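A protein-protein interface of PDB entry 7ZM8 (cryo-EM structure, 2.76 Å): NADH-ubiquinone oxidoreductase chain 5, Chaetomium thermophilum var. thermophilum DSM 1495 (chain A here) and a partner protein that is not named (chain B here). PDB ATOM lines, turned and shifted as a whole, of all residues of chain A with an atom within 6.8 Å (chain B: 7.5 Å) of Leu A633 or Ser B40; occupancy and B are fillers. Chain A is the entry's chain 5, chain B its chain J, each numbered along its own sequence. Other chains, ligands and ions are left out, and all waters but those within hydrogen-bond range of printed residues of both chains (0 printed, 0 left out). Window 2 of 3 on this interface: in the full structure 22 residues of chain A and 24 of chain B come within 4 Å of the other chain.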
ATOM      1  N   VAL A 628     -14.646  20.831   6.748  1.00  0.00           N
ATOM      2  CA  VAL A 628     -15.837  20.024   6.973  1.00  0.00           C
ATOM      3  C   VAL A 628     -15.675  18.637   6.379  1.00  0.00           C
ATOM      4  O   VAL A 628     -16.201  17.660   6.920  1.00  0.00           O
ATOM      5  CB  VAL A 628     -17.079  20.756   6.428  1.00  0.00           C
ATOM      6  CG1 VAL A 628     -17.316  22.003   7.223  1.00  0.00           C
ATOM      7  CG2 VAL A 628     -16.840  21.155   5.001  1.00  0.00           C
ATOM      8  N   THR A 629     -14.962  18.522   5.261  1.00  0.00           N
ATOM      9  CA  THR A 629     -14.735  17.211   4.670  1.00  0.00           C
ATOM     10  C   THR A 629     -13.922  16.317   5.595  1.00  0.00           C
ATOM     11  O   THR A 629     -14.231  15.131   5.743  1.00  0.00           O
ATOM     12  CB  THR A 629     -14.057  17.357   3.307  1.00  0.00           C
ATOM     13  OG1 THR A 629     -12.812  18.049   3.454  1.00  0.00           O
ATOM     14  CG2 THR A 629     -14.948  18.103   2.336  1.00  0.00           C
ATOM     15  N   THR A 630     -12.883  16.860   6.231  1.00  0.00           N
ATOM     16  CA  THR A 630     -12.082  16.034   7.126  1.00  0.00           C
ATOM     17  C   THR A 630     -12.772  15.802   8.466  1.00  0.00           C
ATOM     18  O   THR A 630     -12.540  14.769   9.102  1.00  0.00           O
ATOM     19  CB  THR A 630     -10.689  16.641   7.332  1.00  0.00           C
ATOM     20  OG1 THR A 630      -9.831  15.656   7.913  1.00  0.00           O
ATOM     21  CG2 THR A 630     -10.731  17.805   8.276  1.00  0.00           C
ATOM     22  N   TYR A 631     -13.617  16.733   8.913  1.00  0.00           N
ATOM     23  CA  TYR A 631     -14.359  16.512  10.149  1.00  0.00           C
ATOM     24  C   TYR A 631     -15.413  15.434   9.966  1.00  0.00           C
ATOM     25  O   TYR A 631     -15.672  14.647  10.881  1.00  0.00           O
ATOM     26  CB  TYR A 631     -15.011  17.812  10.618  1.00  0.00           C
ATOM     27  CG  TYR A 631     -14.064  18.795  11.261  1.00  0.00           C
ATOM     28  CD1 TYR A 631     -12.754  18.449  11.541  1.00  0.00           C
ATOM     29  CD2 TYR A 631     -14.486  20.072  11.585  1.00  0.00           C
ATOM     30  CE1 TYR A 631     -11.890  19.351  12.126  1.00  0.00           C
ATOM     31  CE2 TYR A 631     -13.630  20.977  12.167  1.00  0.00           C
ATOM     32  CZ  TYR A 631     -12.334  20.611  12.437  1.00  0.00           C
ATOM     33  OH  TYR A 631     -11.487  21.520  13.016  1.00  0.00           O
ATOM     34  N   ALA A 632     -16.038  15.393   8.790  1.00  0.00           N
ATOM     35  CA  ALA A 632     -17.028  14.365   8.502  1.00  0.00           C
ATOM     36  C   ALA A 632     -16.405  12.979   8.523  1.00  0.00           C
ATOM     37  O   ALA A 632     -17.015  12.021   9.008  1.00  0.00           O
ATOM     38  CB  ALA A 632     -17.669  14.639   7.150  1.00  0.00           C
ATOM     39  N   LEU A 633     -15.187  12.857   7.997  1.00  0.00           N
ATOM     40  CA  LEU A 633     -14.485  11.582   8.030  1.00  0.00           C
ATOM     41  C   LEU A 633     -14.223  11.142   9.462  1.00  0.00           C
ATOM     42  O   LEU A 633     -14.301   9.950   9.777  1.00  0.00           O
ATOM     43  CB  LEU A 633     -13.180  11.704   7.246  1.00  0.00           C
ATOM     44  CG  LEU A 633     -12.543  10.423   6.721  1.00  0.00           C
ATOM     45  CD1 LEU A 633     -13.501   9.711   5.789  1.00  0.00           C
ATOM     46  CD2 LEU A 633     -11.241  10.743   6.007  1.00  0.00           C
ATOM     47  N   TYR A 634     -13.918  12.094  10.345  1.00  0.00           N
ATOM     48  CA  TYR A 634     -13.670  11.768  11.745  1.00  0.00           C
ATOM     49  C   TYR A 634     -14.918  11.215  12.420  1.00  0.00           C
ATOM     50  O   TYR A 634     -14.836  10.265  13.205  1.00  0.00           O
ATOM     51  CB  TYR A 634     -13.174  13.005  12.492  1.00  0.00           C
ATOM     52  CG  TYR A 634     -11.791  13.463  12.110  1.00  0.00           C
ATOM     53  CD1 TYR A 634     -10.942  12.645  11.382  1.00  0.00           C
ATOM     54  CD2 TYR A 634     -11.332  14.716  12.481  1.00  0.00           C
ATOM     55  CE1 TYR A 634      -9.676  13.062  11.035  1.00  0.00           C
ATOM     56  CE2 TYR A 634     -10.064  15.142  12.139  1.00  0.00           C
ATOM     57  CZ  TYR A 634      -9.242  14.309  11.417  1.00  0.00           C
ATOM     58  OH  TYR A 634      -7.982  14.722  11.065  1.00  0.00           O
ATOM     59  N   ILE A 635     -16.079  11.804  12.136  1.00  0.00           N
ATOM     60  CA  ILE A 635     -17.323  11.329  12.737  1.00  0.00           C
ATOM     61  C   ILE A 635     -17.615   9.900  12.310  1.00  0.00           C
ATOM     62  O   ILE A 635     -18.031   9.069  13.124  1.00  0.00           O
ATOM     63  CB  ILE A 635     -18.484  12.276  12.387  1.00  0.00           C
ATOM     64  CG1 ILE A 635     -18.232  13.659  12.978  1.00  0.00           C
ATOM     65  CG2 ILE A 635     -19.799  11.712  12.882  1.00  0.00           C
ATOM     66  CD1 ILE A 635     -19.177  14.712  12.478  1.00  0.00           C
ATOM     67  N   LEU A 636     -17.415   9.590  11.026  1.00  0.00           N
ATOM     68  CA  LEU A 636     -17.575   8.214  10.573  1.00  0.00           C
ATOM     69  C   LEU A 636     -16.585   7.289  11.259  1.00  0.00           C
ATOM     70  O   LEU A 636     -16.945   6.179  11.663  1.00  0.00           O
ATOM     71  CB  LEU A 636     -17.413   8.130   9.058  1.00  0.00           C
ATOM     72  CG  LEU A 636     -18.663   8.246   8.189  1.00  0.00           C
ATOM     73  CD1 LEU A 636     -19.448   6.956   8.300  1.00  0.00           C
ATOM     74  CD2 LEU A 636     -19.527   9.445   8.563  1.00  0.00           C
ATOM     75  N   VAL A 637     -15.334   7.726  11.397  1.00  0.00           N
ATOM     76  CA  VAL A 637     -14.331   6.902  12.060  1.00  0.00           C
ATOM     77  C   VAL A 637     -14.744   6.629  13.496  1.00  0.00           C
ATOM     78  O   VAL A 637     -14.804   5.476  13.936  1.00  0.00           O
ATOM     79  CB  VAL A 637     -12.952   7.578  11.986  1.00  0.00           C
ATOM     80  CG1 VAL A 637     -11.979   6.914  12.947  1.00  0.00           C
ATOM     81  CG2 VAL A 637     -12.422   7.534  10.571  1.00  0.00           C
ATOM     82  N   GLY A 638     -15.081   7.683  14.238  1.00  0.00           N
ATOM     83  CA  GLY A 638     -15.535   7.512  15.605  1.00  0.00           C
ATOM     84  C   GLY A 638     -16.844   6.770  15.716  1.00  0.00           C
ATOM     85  O   GLY A 638     -17.134   6.196  16.769  1.00  0.00           O
ATOM     86  N   PHE A 639     -17.650   6.781  14.653  1.00  0.00           N
ATOM     87  CA  PHE A 639     -18.851   5.957  14.619  1.00  0.00           C
ATOM     88  C   PHE A 639     -18.506   4.478  14.506  1.00  0.00           C
ATOM     89  O   PHE A 639     -19.051   3.652  15.241  1.00  0.00           O
ATOM     90  CB  PHE A 639     -19.739   6.395  13.459  1.00  0.00           C
ATOM     91  CG  PHE A 639     -21.027   5.635  13.355  1.00  0.00           C
ATOM     92  CD1 PHE A 639     -22.072   5.889  14.225  1.00  0.00           C
ATOM     93  CD2 PHE A 639     -21.198   4.672  12.372  1.00  0.00           C
ATOM     94  CE1 PHE A 639     -23.263   5.191  14.125  1.00  0.00           C
ATOM     95  CE2 PHE A 639     -22.380   3.973  12.270  1.00  0.00           C
ATOM     96  CZ  PHE A 639     -23.415   4.234  13.144  1.00  0.00           C
ATOM     97  N   ILE A 640     -17.597   4.127  13.597  1.00  0.00           N
ATOM     98  CA  ILE A 640     -17.266   2.724  13.374  1.00  0.00           C
ATOM     99  C   ILE A 640     -16.613   2.114  14.608  1.00  0.00           C
ATOM    100  O   ILE A 640     -16.881   0.959  14.959  1.00  0.00           O
ATOM    101  CB  ILE A 640     -16.372   2.579  12.129  1.00  0.00           C
ATOM    102  CG1 ILE A 640     -17.040   3.215  10.915  1.00  0.00           C
ATOM    103  CG2 ILE A 640     -16.025   1.124  11.874  1.00  0.00           C
ATOM    104  CD1 ILE A 640     -16.075   3.563   9.808  1.00  0.00           C
ATOM    105  N   PHE B  34      -6.846   2.784  10.951  1.00  0.00           N
ATOM    106  CA  PHE B  34      -6.259   4.096  11.196  1.00  0.00           C
ATOM    107  C   PHE B  34      -5.320   4.500  10.069  1.00  0.00           C
ATOM    108  O   PHE B  34      -5.339   5.649   9.618  1.00  0.00           O
ATOM    109  CB  PHE B  34      -5.526   4.097  12.534  1.00  0.00           C
ATOM    110  CG  PHE B  34      -6.398   4.456  13.696  1.00  0.00           C
ATOM    111  CD1 PHE B  34      -6.990   5.703  13.771  1.00  0.00           C
ATOM    112  CD2 PHE B  34      -6.634   3.545  14.707  1.00  0.00           C
ATOM    113  CE1 PHE B  34      -7.797   6.038  14.837  1.00  0.00           C
ATOM    114  CE2 PHE B  34      -7.440   3.872  15.775  1.00  0.00           C
ATOM    115  CZ  PHE B  34      -8.022   5.121  15.841  1.00  0.00           C
ATOM    116  N   ALA B  35      -4.518   3.564   9.584  1.00  0.00           N
ATOM    117  CA  ALA B  35      -3.631   3.803   8.424  1.00  0.00           C
ATOM    118  C   ALA B  35      -4.466   4.241   7.227  1.00  0.00           C
ATOM    119  O   ALA B  35      -3.977   5.056   6.433  1.00  0.00           O
ATOM    120  CB  ALA B  35      -2.873   2.543   8.122  1.00  0.00           C
ATOM    121  N   ALA B  36      -5.651   3.646   7.070  1.00  0.00           N
ATOM    122  CA  ALA B  36      -6.535   3.953   5.925  1.00  0.00           C
ATOM    123  C   ALA B  36      -6.999   5.410   5.958  1.00  0.00           C
ATOM    124  O   ALA B  36      -7.128   6.004   4.899  1.00  0.00           O
ATOM    125  CB  ALA B  36      -7.679   2.990   5.915  1.00  0.00           C
ATOM    126  N   VAL B  37      -7.287   5.938   7.139  1.00  0.00           N
ATOM    127  CA  VAL B  37      -7.698   7.360   7.295  1.00  0.00           C
ATOM    128  C   VAL B  37      -6.535   8.225   6.831  1.00  0.00           C
ATOM    129  O   VAL B  37      -6.787   9.255   6.200  1.00  0.00           O
ATOM    130  CB  VAL B  37      -8.057   7.637   8.763  1.00  0.00           C
ATOM    131  CG1 VAL B  37      -8.544   9.062   8.975  1.00  0.00           C
ATOM    132  CG2 VAL B  37      -9.088   6.647   9.270  1.00  0.00           C
ATOM    133  N   ARG B  38      -5.309   7.811   7.144  1.00  0.00           N
ATOM    134  CA  ARG B  38      -4.097   8.580   6.779  1.00  0.00           C
ATOM    135  C   ARG B  38      -3.988   8.648   5.261  1.00  0.00           C
ATOM    136  O   ARG B  38      -3.592   9.695   4.748  1.00  0.00           O
ATOM    137  CB  ARG B  38      -2.902   7.885   7.423  1.00  0.00           C
ATOM    138  CG  ARG B  38      -2.773   8.127   8.919  1.00  0.00           C
ATOM    139  CD  ARG B  38      -2.076   9.445   9.188  1.00  0.00           C
ATOM    140  NE  ARG B  38      -0.747   9.471   8.593  1.00  0.00           N
ATOM    141  CZ  ARG B  38       0.370   9.144   9.232  1.00  0.00           C
ATOM    142  NH1 ARG B  38       0.323   8.772  10.499  1.00  0.00           N
ATOM    143  NH2 ARG B  38       1.530   9.197   8.603  1.00  0.00           N
ATOM    144  N   THR B  39      -4.285   7.541   4.590  1.00  0.00           N
ATOM    145  CA  THR B  39      -4.244   7.480   3.114  1.00  0.00           C
ATOM    146  C   THR B  39      -5.333   8.384   2.551  1.00  0.00           C
ATOM    147  O   THR B  39      -5.021   9.187   1.665  1.00  0.00           O
ATOM    148  CB  THR B  39      -4.399   6.024   2.668  1.00  0.00           C
ATOM    149  OG1 THR B  39      -3.783   5.198   3.656  1.00  0.00           O
ATOM    150  CG2 THR B  39      -3.786   5.749   1.312  1.00  0.00           C
ATOM    151  N   SER B  40      -6.536   8.303   3.109  1.00  0.00           N
ATOM    152  CA  SER B  40      -7.682   9.119   2.631  1.00  0.00           C
ATOM    153  C   SER B  40      -7.396  10.596   2.839  1.00  0.00           C
ATOM    154  O   SER B  40      -7.812  11.393   1.986  1.00  0.00           O
ATOM    155  CB  SER B  40      -8.932   8.724   3.330  1.00  0.00           C
ATOM    156  OG  SER B  40     -10.070   9.181   2.619  1.00  0.00           O
ATOM    157  N   LEU B  41      -6.744  10.938   3.949  1.00  0.00           N
ATOM    158  CA  LEU B  41      -6.502  12.360   4.280  1.00  0.00           C
ATOM    159  C   LEU B  41      -5.211  12.868   3.645  1.00  0.00           C
ATOM    160  O   LEU B  41      -4.965  14.074   3.753  1.00  0.00           O
ATOM    161  CB  LEU B  41      -6.519  12.536   5.796  1.00  0.00           C
ATOM    162  CG  LEU B  41      -7.916  12.570   6.409  1.00  0.00           C
ATOM    163  CD1 LEU B  41      -7.857  12.988   7.867  1.00  0.00           C
ATOM    164  CD2 LEU B  41      -8.821  13.498   5.619  1.00  0.00           C
ATOM    165  N   ALA B  42      -4.447  12.005   2.976  1.00  0.00           N
ATOM    166  CA  ALA B  42      -3.184  12.460   2.415  1.00  0.00           C
ATOM    167  C   ALA B  42      -3.431  13.521   1.352  1.00  0.00           C
ATOM    168  O   ALA B  42      -4.357  13.413   0.544  1.00  0.00           O
ATOM    169  CB  ALA B  42      -2.412  11.284   1.821  1.00  0.00           C
ATOM    170  N   ARG B  43      -2.591  14.549   1.354  1.00  0.00           N
ATOM    171  CA  ARG B  43      -2.795  15.723   0.519  1.00  0.00           C
ATOM    172  C   ARG B  43      -2.141  15.609  -0.853  1.00  0.00           C
ATOM    173  O   ARG B  43      -2.211  16.564  -1.634  1.00  0.00           O
ATOM    174  CB  ARG B  43      -2.272  16.964   1.243  1.00  0.00           C
ATOM    175  CG  ARG B  43      -2.850  17.130   2.640  1.00  0.00           C
ATOM    176  CD  ARG B  43      -2.364  18.401   3.316  1.00  0.00           C
ATOM    177  NE  ARG B  43      -2.700  18.408   4.738  1.00  0.00           N
ATOM    178  CZ  ARG B  43      -3.879  18.777   5.228  1.00  0.00           C
ATOM    179  NH1 ARG B  43      -4.094  18.748   6.536  1.00  0.00           N
ATOM    180  NH2 ARG B  43      -4.844  19.175   4.411  1.00  0.00           N
ATOM    181  N   LYS B  44      -1.509  14.483  -1.163  1.00  0.00           N
ATOM    182  CA  LYS B  44      -0.888  14.259  -2.459  1.00  0.00           C
ATOM    183  C   LYS B  44      -1.422  12.972  -3.074  1.00  0.00           C
ATOM    184  O   LYS B  44      -2.055  12.149  -2.406  1.00  0.00           O
ATOM    185  CB  LYS B  44       0.639  14.201  -2.339  1.00  0.00           C
ATOM    186  CG  LYS B  44       1.285  15.540  -2.026  1.00  0.00           C
ATOM    187  CD  LYS B  44       2.798  15.425  -1.986  1.00  0.00           C
ATOM    188  CE  LYS B  44       3.365  15.193  -3.375  1.00  0.00           C
ATOM    189  NZ  LYS B  44       3.154  16.370  -4.262  1.00  0.00           N
ATOM    190  N   VAL B  46      -0.986   9.917  -3.553  1.00  0.00           N
ATOM    191  CA  VAL B  46      -0.225   8.768  -3.080  1.00  0.00           C
ATOM    192  C   VAL B  46      -0.808   7.446  -3.559  1.00  0.00           C
ATOM    193  O   VAL B  46      -0.115   6.423  -3.518  1.00  0.00           O
ATOM    194  CB  VAL B  46      -0.135   8.781  -1.546  1.00  0.00           C
ATOM    195  CG1 VAL B  46       0.598  10.024  -1.075  1.00  0.00           C
ATOM    196  CG2 VAL B  46      -1.528   8.730  -0.943  1.00  0.00           C
ATOM    197  N   GLY B  47      -2.060   7.435  -4.007  1.00  0.00           N
ATOM    198  CA  GLY B  47      -2.662   6.245  -4.559  1.00  0.00           C
ATOM    199  C   GLY B  47      -3.163   5.283  -3.504  1.00  0.00           C
ATOM    200  O   GLY B  47      -3.104   5.552  -2.301  1.00  0.00           O
ATOM    201  N   ASN B  55       2.017   4.320   5.313  1.00  0.00           N
ATOM    202  CA  ASN B  55       1.353   4.142   6.598  1.00  0.00           C
ATOM    203  C   ASN B  55       1.436   2.710   7.109  1.00  0.00           C
ATOM    204  O   ASN B  55       0.768   2.377   8.092  1.00  0.00           O
ATOM    205  CB  ASN B  55      -0.112   4.571   6.509  1.00  0.00           C
ATOM    206  CG  ASN B  55      -0.285   5.918   5.853  1.00  0.00           C
ATOM    207  OD1 ASN B  55      -1.021   6.056   4.880  1.00  0.00           O
ATOM    208  ND2 ASN B  55       0.388   6.925   6.389  1.00  0.00           N
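Among the printed residues, merely in contact across the chains: Thr A630 with Leu B41, Leu A633 with Ser B40, Leu A633 with Leu B41, Tyr A634 with Leu B41 and Val A637 with Val B37.
Hydrophobic or aromatic side chains of chain A that line the printed part of chain B: Leu A633, Tyr A634 and Val A637. Printed residues of chain B that touch a printed residue of chain A: Val B37, Ser B40 and Leu B41. Hydrophobic or aromatic side chains of chain B that line the printed part of chain A: Val B37 and Leu B41. Among the printed residues, 5 pairs touch across the chains.
Leu A633 touches two residues of chain B. Ser B40 touches one residue of chain A. No residue of chain B comes within 4 Å of Ala A632. Of the printed residues of chain A, Val B37 touches Val A637. Of the printed residues of chain A, Leu B41 touches Thr A630 (3.3 Å), Leu A633 (3.7 Å) and Tyr A634 (3.6 Å). Of the printed residues of chain B, Val A637 touches Val B37. Printed residues of chain B within 4 Å of Thr A630: Leu B41. Gly A638 touches none of the printed residues of chain B. Val B46 touches none of the printed residues of chain A. The nearest printed residue of chain A that does not touch Ser B40 is Thr A630 (7.6 Å). The nearest printed residue of chain A that does not touch Leu B41 is Thr A629 (5.7 Å).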
